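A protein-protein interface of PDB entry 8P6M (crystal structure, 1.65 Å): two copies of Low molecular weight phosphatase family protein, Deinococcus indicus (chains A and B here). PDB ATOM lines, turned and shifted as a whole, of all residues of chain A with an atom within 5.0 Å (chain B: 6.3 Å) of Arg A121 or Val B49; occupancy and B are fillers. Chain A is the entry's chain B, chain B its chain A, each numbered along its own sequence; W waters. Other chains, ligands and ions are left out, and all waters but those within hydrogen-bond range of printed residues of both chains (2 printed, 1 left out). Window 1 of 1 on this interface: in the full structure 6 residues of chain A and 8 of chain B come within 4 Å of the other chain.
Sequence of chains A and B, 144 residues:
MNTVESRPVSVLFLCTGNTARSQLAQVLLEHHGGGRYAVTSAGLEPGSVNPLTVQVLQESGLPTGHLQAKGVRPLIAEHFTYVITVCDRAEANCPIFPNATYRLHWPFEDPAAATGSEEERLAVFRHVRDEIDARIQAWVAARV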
ATOM      1  N   LEU A  52      22.705  32.314 -11.991  1.00  0.00           N
ATOM      2  CA  LEU A  52      22.201  33.646 -12.297  1.00  0.00           C
ATOM      3  C   LEU A  52      22.830  34.710 -11.400  1.00  0.00           C
ATOM      4  O   LEU A  52      22.984  35.863 -11.828  1.00  0.00           O
ATOM      5  CB  LEU A  52      20.675  33.658 -12.177  1.00  0.00           C
ATOM      6  CG  LEU A  52      20.008  32.613 -13.070  1.00  0.00           C
ATOM      7  CD1 LEU A  52      18.489  32.719 -12.973  1.00  0.00           C
ATOM      8  CD2 LEU A  52      20.457  32.785 -14.504  1.00  0.00           C
ATOM      9  N   ALA A 114      12.155  33.526  -8.012  1.00  0.00           N
ATOM     10  CA  ALA A 114      11.508  33.914  -9.257  1.00  0.00           C
ATOM     11  C   ALA A 114      11.422  32.729 -10.209  1.00  0.00           C
ATOM     12  O   ALA A 114      12.372  31.955 -10.352  1.00  0.00           O
ATOM     13  CB  ALA A 114      12.274  35.062  -9.914  1.00  0.00           C
ATOM     14  N   THR A 115      10.271  32.589 -10.856  1.00  0.00           N
ATOM     15  CA  THR A 115      10.055  31.584 -11.883  1.00  0.00           C
ATOM     16  C   THR A 115      10.038  32.258 -13.253  1.00  0.00           C
ATOM     17  O   THR A 115      10.262  33.465 -13.387  1.00  0.00           O
ATOM     18  CB  THR A 115       8.756  30.821 -11.623  1.00  0.00           C
ATOM     19  OG1 THR A 115       7.650  31.725 -11.717  1.00  0.00           O
ATOM     20  CG2 THR A 115       8.779  30.194 -10.232  1.00  0.00           C
ATOM     21  N   GLY A 116       9.782  31.461 -14.278  1.00  0.00           N
ATOM     22  CA  GLY A 116       9.747  31.956 -15.638  1.00  0.00           C
ATOM     23  C   GLY A 116      11.023  31.637 -16.393  1.00  0.00           C
ATOM     24  O   GLY A 116      11.904  30.908 -15.927  1.00  0.00           O
ATOM     25  N   SER A 117      11.113  32.219 -17.586  1.00  0.00           N
ATOM     26  CA  SER A 117      12.250  32.023 -18.471  1.00  0.00           C
ATOM     27  C   SER A 117      13.527  32.582 -17.850  1.00  0.00           C
ATOM     28  O   SER A 117      13.502  33.331 -16.872  1.00  0.00           O
ATOM     29  CB  SER A 117      12.005  32.717 -19.806  1.00  0.00           C
ATOM     30  OG  SER A 117      12.030  34.124 -19.614  1.00  0.00           O
ATOM     31  N   GLU A 118      14.662  32.244 -18.470  1.00  0.00           N
ATOM     32  CA  GLU A 118      15.931  32.769 -17.981  1.00  0.00           C
ATOM     33  C   GLU A 118      15.936  34.293 -17.984  1.00  0.00           C
ATOM     34  O   GLU A 118      16.400  34.916 -17.025  1.00  0.00           O
ATOM     35  CB  GLU A 118      17.103  32.235 -18.802  1.00  0.00           C
ATOM     36  CG  GLU A 118      18.462  32.659 -18.221  1.00  0.00           C
ATOM     37  CD  GLU A 118      19.643  32.134 -19.016  1.00  0.00           C
ATOM     38  OE1 GLU A 118      19.852  32.597 -20.164  1.00  0.00           O
ATOM     39  OE2 GLU A 118      20.359  31.254 -18.492  1.00  0.00           O
ATOM     40  N   GLU A 119      15.411  34.913 -19.048  1.00  0.00           N
ATOM     41  CA  GLU A 119      15.367  36.375 -19.104  1.00  0.00           C
ATOM     42  C   GLU A 119      14.536  36.949 -17.963  1.00  0.00           C
ATOM     43  O   GLU A 119      14.919  37.953 -17.346  1.00  0.00           O
ATOM     44  CB  GLU A 119      14.807  36.842 -20.448  1.00  0.00           C
ATOM     45  CG  GLU A 119      14.705  38.357 -20.593  1.00  0.00           C
ATOM     46  CD  GLU A 119      13.936  38.779 -21.837  1.00  0.00           C
ATOM     47  OE1 GLU A 119      13.130  37.970 -22.347  1.00  0.00           O
ATOM     48  OE2 GLU A 119      14.138  39.920 -22.306  1.00  0.00           O
ATOM     49  N   GLU A 120      13.388  36.335 -17.680  1.00  0.00           N
ATOM     50  CA  GLU A 120      12.527  36.846 -16.618  1.00  0.00           C
ATOM     51  C   GLU A 120      13.198  36.708 -15.258  1.00  0.00           C
ATOM     52  O   GLU A 120      13.135  37.626 -14.430  1.00  0.00           O
ATOM     53  CB  GLU A 120      11.176  36.125 -16.651  1.00  0.00           C
ATOM     54  CG  GLU A 120      10.369  36.401 -17.924  1.00  0.00           C
ATOM     55  CD  GLU A 120       9.093  35.574 -18.028  1.00  0.00           C
ATOM     56  OE1 GLU A 120       9.159  34.336 -17.862  1.00  0.00           O
ATOM     57  OE2 GLU A 120       8.022  36.163 -18.290  1.00  0.00           O
ATOM     58  N   ARG A 121      13.878  35.583 -15.020  1.00  0.00           N
ATOM     59  CA  ARG A 121      14.586  35.409 -13.759  1.00  0.00           C
ATOM     60  C   ARG A 121      15.760  36.372 -13.654  1.00  0.00           C
ATOM     61  O   ARG A 121      15.967  36.995 -12.604  1.00  0.00           O
ATOM     62  CB  ARG A 121      15.054  33.959 -13.627  1.00  0.00           C
ATOM     63  CG  ARG A 121      13.924  32.947 -13.663  1.00  0.00           C
ATOM     64  CD  ARG A 121      14.428  31.554 -13.309  1.00  0.00           C
ATOM     65  NE  ARG A 121      13.417  30.527 -13.520  1.00  0.00           N
ATOM     66  CZ  ARG A 121      13.485  29.300 -13.025  1.00  0.00           C
ATOM     67  NH1 ARG A 121      14.475  28.933 -12.224  1.00  0.00           N
ATOM     68  NH2 ARG A 121      12.540  28.419 -13.342  1.00  0.00           N
ATOM     69  N   LEU A 122      16.522  36.529 -14.743  1.00  0.00           N
ATOM     70  CA  LEU A 122      17.652  37.451 -14.735  1.00  0.00           C
ATOM     71  C   LEU A 122      17.215  38.884 -14.452  1.00  0.00           C
ATOM     72  O   LEU A 122      17.983  39.654 -13.871  1.00  0.00           O
ATOM     73  CB  LEU A 122      18.406  37.386 -16.064  1.00  0.00           C
ATOM     74  CG  LEU A 122      19.402  36.234 -16.241  1.00  0.00           C
ATOM     75  CD1 LEU A 122      19.930  36.191 -17.665  1.00  0.00           C
ATOM     76  CD2 LEU A 122      20.557  36.364 -15.256  1.00  0.00           C
ATOM     77  N   ALA A 123      16.004  39.271 -14.868  1.00  0.00           N
ATOM     78  CA  ALA A 123      15.502  40.601 -14.539  1.00  0.00           C
ATOM     79  C   ALA A 123      15.381  40.794 -13.030  1.00  0.00           C
ATOM     80  O   ALA A 123      15.723  41.861 -12.501  1.00  0.00           O
ATOM     81  CB  ALA A 123      14.150  40.828 -15.214  1.00  0.00           C
ATOM     82  N   VAL A 124      14.890  39.781 -12.318  1.00  0.00           N
ATOM     83  CA  VAL A 124      14.779  39.906 -10.866  1.00  0.00           C
ATOM     84  C   VAL A 124      16.158  39.922 -10.225  1.00  0.00           C
ATOM     85  O   VAL A 124      16.426  40.726  -9.322  1.00  0.00           O
ATOM     86  CB  VAL A 124      13.900  38.783 -10.287  1.00  0.00           C
ATOM     87  CG1 VAL A 124      13.791  38.926  -8.763  1.00  0.00           C
ATOM     88  CG2 VAL A 124      12.532  38.788 -10.954  1.00  0.00           C
ATOM     89  N   PHE A 125      17.061  39.049 -10.691  1.00  0.00           N
ATOM     90  CA  PHE A 125      18.420  39.021 -10.153  1.00  0.00           C
ATOM     91  C   PHE A 125      19.114  40.365 -10.343  1.00  0.00           C
ATOM     92  O   PHE A 125      19.825  40.836  -9.447  1.00  0.00           O
ATOM     93  CB  PHE A 125      19.233  37.898 -10.810  1.00  0.00           C
ATOM     94  CG  PHE A 125      19.133  36.569 -10.098  1.00  0.00           C
ATOM     95  CD1 PHE A 125      18.125  35.666 -10.409  1.00  0.00           C
ATOM     96  CD2 PHE A 125      20.067  36.210  -9.134  1.00  0.00           C
ATOM     97  CE1 PHE A 125      18.038  34.438  -9.761  1.00  0.00           C
ATOM     98  CE2 PHE A 125      19.980  34.992  -8.476  1.00  0.00           C
ATOM     99  CZ  PHE A 125      18.961  34.097  -8.801  1.00  0.00           C
ATOM    100  N   ASN B  18      20.911  18.707  -8.725  1.00  0.00           N
ATOM    101  CA  ASN B  18      19.473  18.486  -8.911  1.00  0.00           C
ATOM    102  C   ASN B  18      18.838  19.646  -9.685  1.00  0.00           C
ATOM    103  O   ASN B  18      17.710  20.058  -9.415  1.00  0.00           O
ATOM    104  CB  ASN B  18      18.773  18.244  -7.566  1.00  0.00           C
ATOM    105  CG  ASN B  18      17.373  17.627  -7.714  1.00  0.00           C
ATOM    106  OD1 ASN B  18      16.467  17.957  -6.952  1.00  0.00           O
ATOM    107  ND2 ASN B  18      17.199  16.744  -8.690  1.00  0.00           N
ATOM    108  N   THR B  19      19.581  20.191 -10.658  1.00  0.00           N
ATOM    109  CA  THR B  19      19.083  21.297 -11.465  1.00  0.00           C
ATOM    110  C   THR B  19      18.795  20.941 -12.915  1.00  0.00           C
ATOM    111  O   THR B  19      18.079  21.701 -13.576  1.00  0.00           O
ATOM    112  CB  THR B  19      20.075  22.474 -11.474  1.00  0.00           C
ATOM    113  OG1 THR B  19      21.133  22.200 -12.402  1.00  0.00           O
ATOM    114  CG2 THR B  19      20.658  22.711 -10.082  1.00  0.00           C
ATOM    115  N   ALA B  20      19.351  19.838 -13.440  1.00  0.00           N
ATOM    116  CA  ALA B  20      19.218  19.570 -14.871  1.00  0.00           C
ATOM    117  C   ALA B  20      19.062  18.087 -15.192  1.00  0.00           C
ATOM    118  O   ALA B  20      17.937  17.614 -15.366  1.00  0.00           O
ATOM    119  CB  ALA B  20      20.415  20.142 -15.638  1.00  0.00           C
ATOM    120  N   GLN B  23      16.719  16.075 -13.069  1.00  0.00           N
ATOM    121  CA  GLN B  23      15.366  16.594 -13.259  1.00  0.00           C
ATOM    122  C   GLN B  23      14.784  16.141 -14.590  1.00  0.00           C
ATOM    123  O   GLN B  23      13.611  15.749 -14.665  1.00  0.00           O
ATOM    124  CB  GLN B  23      15.377  18.124 -13.183  1.00  0.00           C
ATOM    125  CG  GLN B  23      15.823  18.692 -11.844  1.00  0.00           C
ATOM    126  CD  GLN B  23      14.792  18.536 -10.749  1.00  0.00           C
ATOM    127  OE1 GLN B  23      13.683  18.042 -10.982  1.00  0.00           O
ATOM    128  NE2 GLN B  23      15.142  18.971  -9.539  1.00  0.00           N
ATOM    129  N   GLY B  47      20.992  22.974  -5.889  1.00  0.00           N
ATOM    130  CA  GLY B  47      20.975  24.336  -6.374  1.00  0.00           C
ATOM    131  C   GLY B  47      19.559  24.822  -6.604  1.00  0.00           C
ATOM    132  O   GLY B  47      18.753  24.887  -5.671  1.00  0.00           O
ATOM    133  N   SER B  48      19.254  25.158  -7.851  1.00  0.00           N
ATOM    134  CA  SER B  48      17.951  25.670  -8.242  1.00  0.00           C
ATOM    135  C   SER B  48      17.684  25.160  -9.650  1.00  0.00           C
ATOM    136  O   SER B  48      18.602  25.100 -10.469  1.00  0.00           O
ATOM    137  CB  SER B  48      17.922  27.205  -8.178  1.00  0.00           C
ATOM    138  OG  SER B  48      16.656  27.725  -8.553  1.00  0.00           O
ATOM    139  N   VAL B  49      16.441  24.763  -9.923  1.00  0.00           N
ATOM    140  CA  VAL B  49      16.128  24.214 -11.238  1.00  0.00           C
ATOM    141  C   VAL B  49      16.486  25.232 -12.315  1.00  0.00           C
ATOM    142  O   VAL B  49      16.062  26.391 -12.260  1.00  0.00           O
ATOM    143  CB  VAL B  49      14.647  23.817 -11.325  1.00  0.00           C
ATOM    144  CG1 VAL B  49      14.328  23.328 -12.724  1.00  0.00           C
ATOM    145  CG2 VAL B  49      14.310  22.749 -10.306  1.00  0.00           C
ATOM    146  N   ASN B  50      17.284  24.805 -13.289  1.00  0.00           N
ATOM    147  CA  ASN B  50      17.712  25.709 -14.357  1.00  0.00           C
ATOM    148  C   ASN B  50      16.515  26.063 -15.234  1.00  0.00           C
ATOM    149  O   ASN B  50      15.758  25.166 -15.625  1.00  0.00           O
ATOM    150  CB  ASN B  50      18.822  25.040 -15.181  1.00  0.00           C
ATOM    151  CG  ASN B  50      19.551  26.001 -16.109  1.00  0.00           C
ATOM    152  OD1 ASN B  50      18.935  26.701 -16.904  1.00  0.00           O
ATOM    153  ND2 ASN B  50      20.882  26.020 -16.018  1.00  0.00           N
ATOM    154  N   PRO B  51      16.304  27.343 -15.562  1.00  0.00           N
ATOM    155  CA  PRO B  51      15.180  27.690 -16.455  1.00  0.00           C
ATOM    156  C   PRO B  51      15.219  26.971 -17.793  1.00  0.00           C
ATOM    157  O   PRO B  51      14.162  26.699 -18.376  1.00  0.00           O
ATOM    158  CB  PRO B  51      15.323  29.210 -16.631  1.00  0.00           C
ATOM    159  CG  PRO B  51      16.734  29.535 -16.206  1.00  0.00           C
ATOM    160  CD  PRO B  51      17.055  28.536 -15.123  1.00  0.00           C
ATOM    161  N   LEU B  52      16.406  26.647 -18.303  1.00  0.00           N
ATOM    162  CA  LEU B  52      16.491  25.946 -19.582  1.00  0.00           C
ATOM    163  C   LEU B  52      16.044  24.495 -19.457  1.00  0.00           C
ATOM    164  O   LEU B  52      15.546  23.913 -20.432  1.00  0.00           O
ATOM    165  CB  LEU B  52      17.918  26.020 -20.120  1.00  0.00           C
ATOM    166  CG  LEU B  52      18.327  27.345 -20.769  1.00  0.00           C
ATOM    167  CD1 LEU B  52      18.271  28.561 -19.837  1.00  0.00           C
ATOM    168  CD2 LEU B  52      19.731  27.216 -21.372  1.00  0.00           C
ATOM    169  N   THR B  53      16.237  23.893 -18.281  1.00  0.00           N
ATOM    170  CA  THR B  53      15.697  22.564 -18.024  1.00  0.00           C
ATOM    171  C   THR B  53      14.189  22.568 -18.185  1.00  0.00           C
ATOM    172  O   THR B  53      13.616  21.713 -18.870  1.00  0.00           O
ATOM    173  CB  THR B  53      16.067  22.123 -16.612  1.00  0.00           C
ATOM    174  OG1 THR B  53      17.488  22.214 -16.450  1.00  0.00           O
ATOM    175  CG2 THR B  53      15.597  20.691 -16.342  1.00  0.00           C
ATOM    176  N   VAL B  54      13.536  23.533 -17.536  1.00  0.00           N
ATOM    177  CA  VAL B  54      12.088  23.679 -17.631  1.00  0.00           C
ATOM    178  C   VAL B  54      11.676  23.940 -19.074  1.00  0.00           C
ATOM    179  O   VAL B  54      10.714  23.346 -19.576  1.00  0.00           O
ATOM    180  CB  VAL B  54      11.614  24.798 -16.688  1.00  0.00           C
ATOM    181  CG1 VAL B  54      10.200  25.236 -17.034  1.00  0.00           C
ATOM    182  CG2 VAL B  54      11.697  24.335 -15.227  1.00  0.00           C
ATOM    183  N   LEU B  67       8.738  20.486  -9.975  1.00  0.00           N
ATOM    184  CA  LEU B  67      10.179  20.295  -9.883  1.00  0.00           C
ATOM    185  C   LEU B  67      10.766  21.227  -8.831  1.00  0.00           C
ATOM    186  O   LEU B  67      10.411  22.408  -8.762  1.00  0.00           O
ATOM    187  CB  LEU B  67      10.848  20.535 -11.236  1.00  0.00           C
ATOM    188  CG  LEU B  67      10.339  19.719 -12.424  1.00  0.00           C
ATOM    189  CD1 LEU B  67      11.264  19.892 -13.621  1.00  0.00           C
ATOM    190  CD2 LEU B  67      10.227  18.260 -12.028  1.00  0.00           C
ATOM    191  N   GLN B  68      11.650  20.676  -8.003  1.00  0.00           N
ATOM    192  CA  GLN B  68      12.392  21.405  -6.980  1.00  0.00           C
ATOM    193  C   GLN B  68      13.785  20.804  -6.903  1.00  0.00           C
ATOM    194  O   GLN B  68      13.928  19.578  -6.886  1.00  0.00           O
ATOM    195  CB  GLN B  68      11.736  21.300  -5.599  1.00  0.00           C
ATOM    196  CG  GLN B  68      10.284  21.689  -5.507  1.00  0.00           C
ATOM    197  CD  GLN B  68       9.763  21.560  -4.089  1.00  0.00           C
ATOM    198  OE1 GLN B  68       9.179  20.540  -3.719  1.00  0.00           O
ATOM    199  NE2 GLN B  68       9.989  22.591  -3.281  1.00  0.00           N
ATOM    200  N   ALA B  69      14.807  21.655  -6.856  1.00  0.00           N
ATOM    201  CA  ALA B  69      16.152  21.172  -6.579  1.00  0.00           C
ATOM    202  C   ALA B  69      16.258  20.823  -5.100  1.00  0.00           C
ATOM    203  O   ALA B  69      16.023  21.675  -4.234  1.00  0.00           O
ATOM    204  CB  ALA B  69      17.189  22.222  -6.966  1.00  0.00           C
HETATM  205  O   HOH W   1      19.938  29.427 -16.470  1.00  0.00           O
HETATM  206  O   HOH W   2      11.859  28.353 -18.212  1.00  0.00           O
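Printed residues of chain A that touch a printed residue of chain B: Gly A116, Glu A118 and Arg A121.
Among the printed residues, 5 pairs touch across the chains.
Among the printed residues, merely in contact across the chains: Glu A118 with Pro B51, Glu A118 with Leu B52, Arg A121 with Pro B51 and Gly A116 with Pro B51.
Of the printed residues of chain B, Arg A121 touches Val B49 (3.0 Å) and Pro B51 (3.9 Å).
Val B49 touches just one residue of chain A: Arg A121.
Of the printed residues of chain A, Leu B52 touches Glu A118 (3.7 Å).
Printed residues of chain B within 4 Å of Glu A118: Pro B51 and Leu B52.
Val A124 touches none of the printed residues of chain B.
The nearest residue of chain B that does not touch Arg A121 is Ser B48 (4.4 Å).
Water W1 lies within hydrogen-bond range of the side-chain carboxylate of Glu A118 (2.8 Å) and the side-chain amide oxygen of Asn B50 (2.9 Å).
Water W2 lies within hydrogen-bond range of the backbone carbonyl oxygen (O) of Pro B51 (2.8 Å) and the backbone carbonyl oxygen (O) of Gly A116 (3.4 Å).
The side-chain amide oxygen of Asn B50 lies within hydrogen-bond range of the backbone NH of Leu B52 (2.9 Å).
NE of Arg A121 is in hydrogen-bond range of O of Gly A116 (2.9 Å).
The guanidinium group of Arg A121 is in hydrogen-bond range of the backbone carbonyl oxygen of Val B49.
Position printed for both chains: 52.
Of the 5 pairs that touch across the chains among the printed residues, none has its exchanged pair printed and touching as well.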
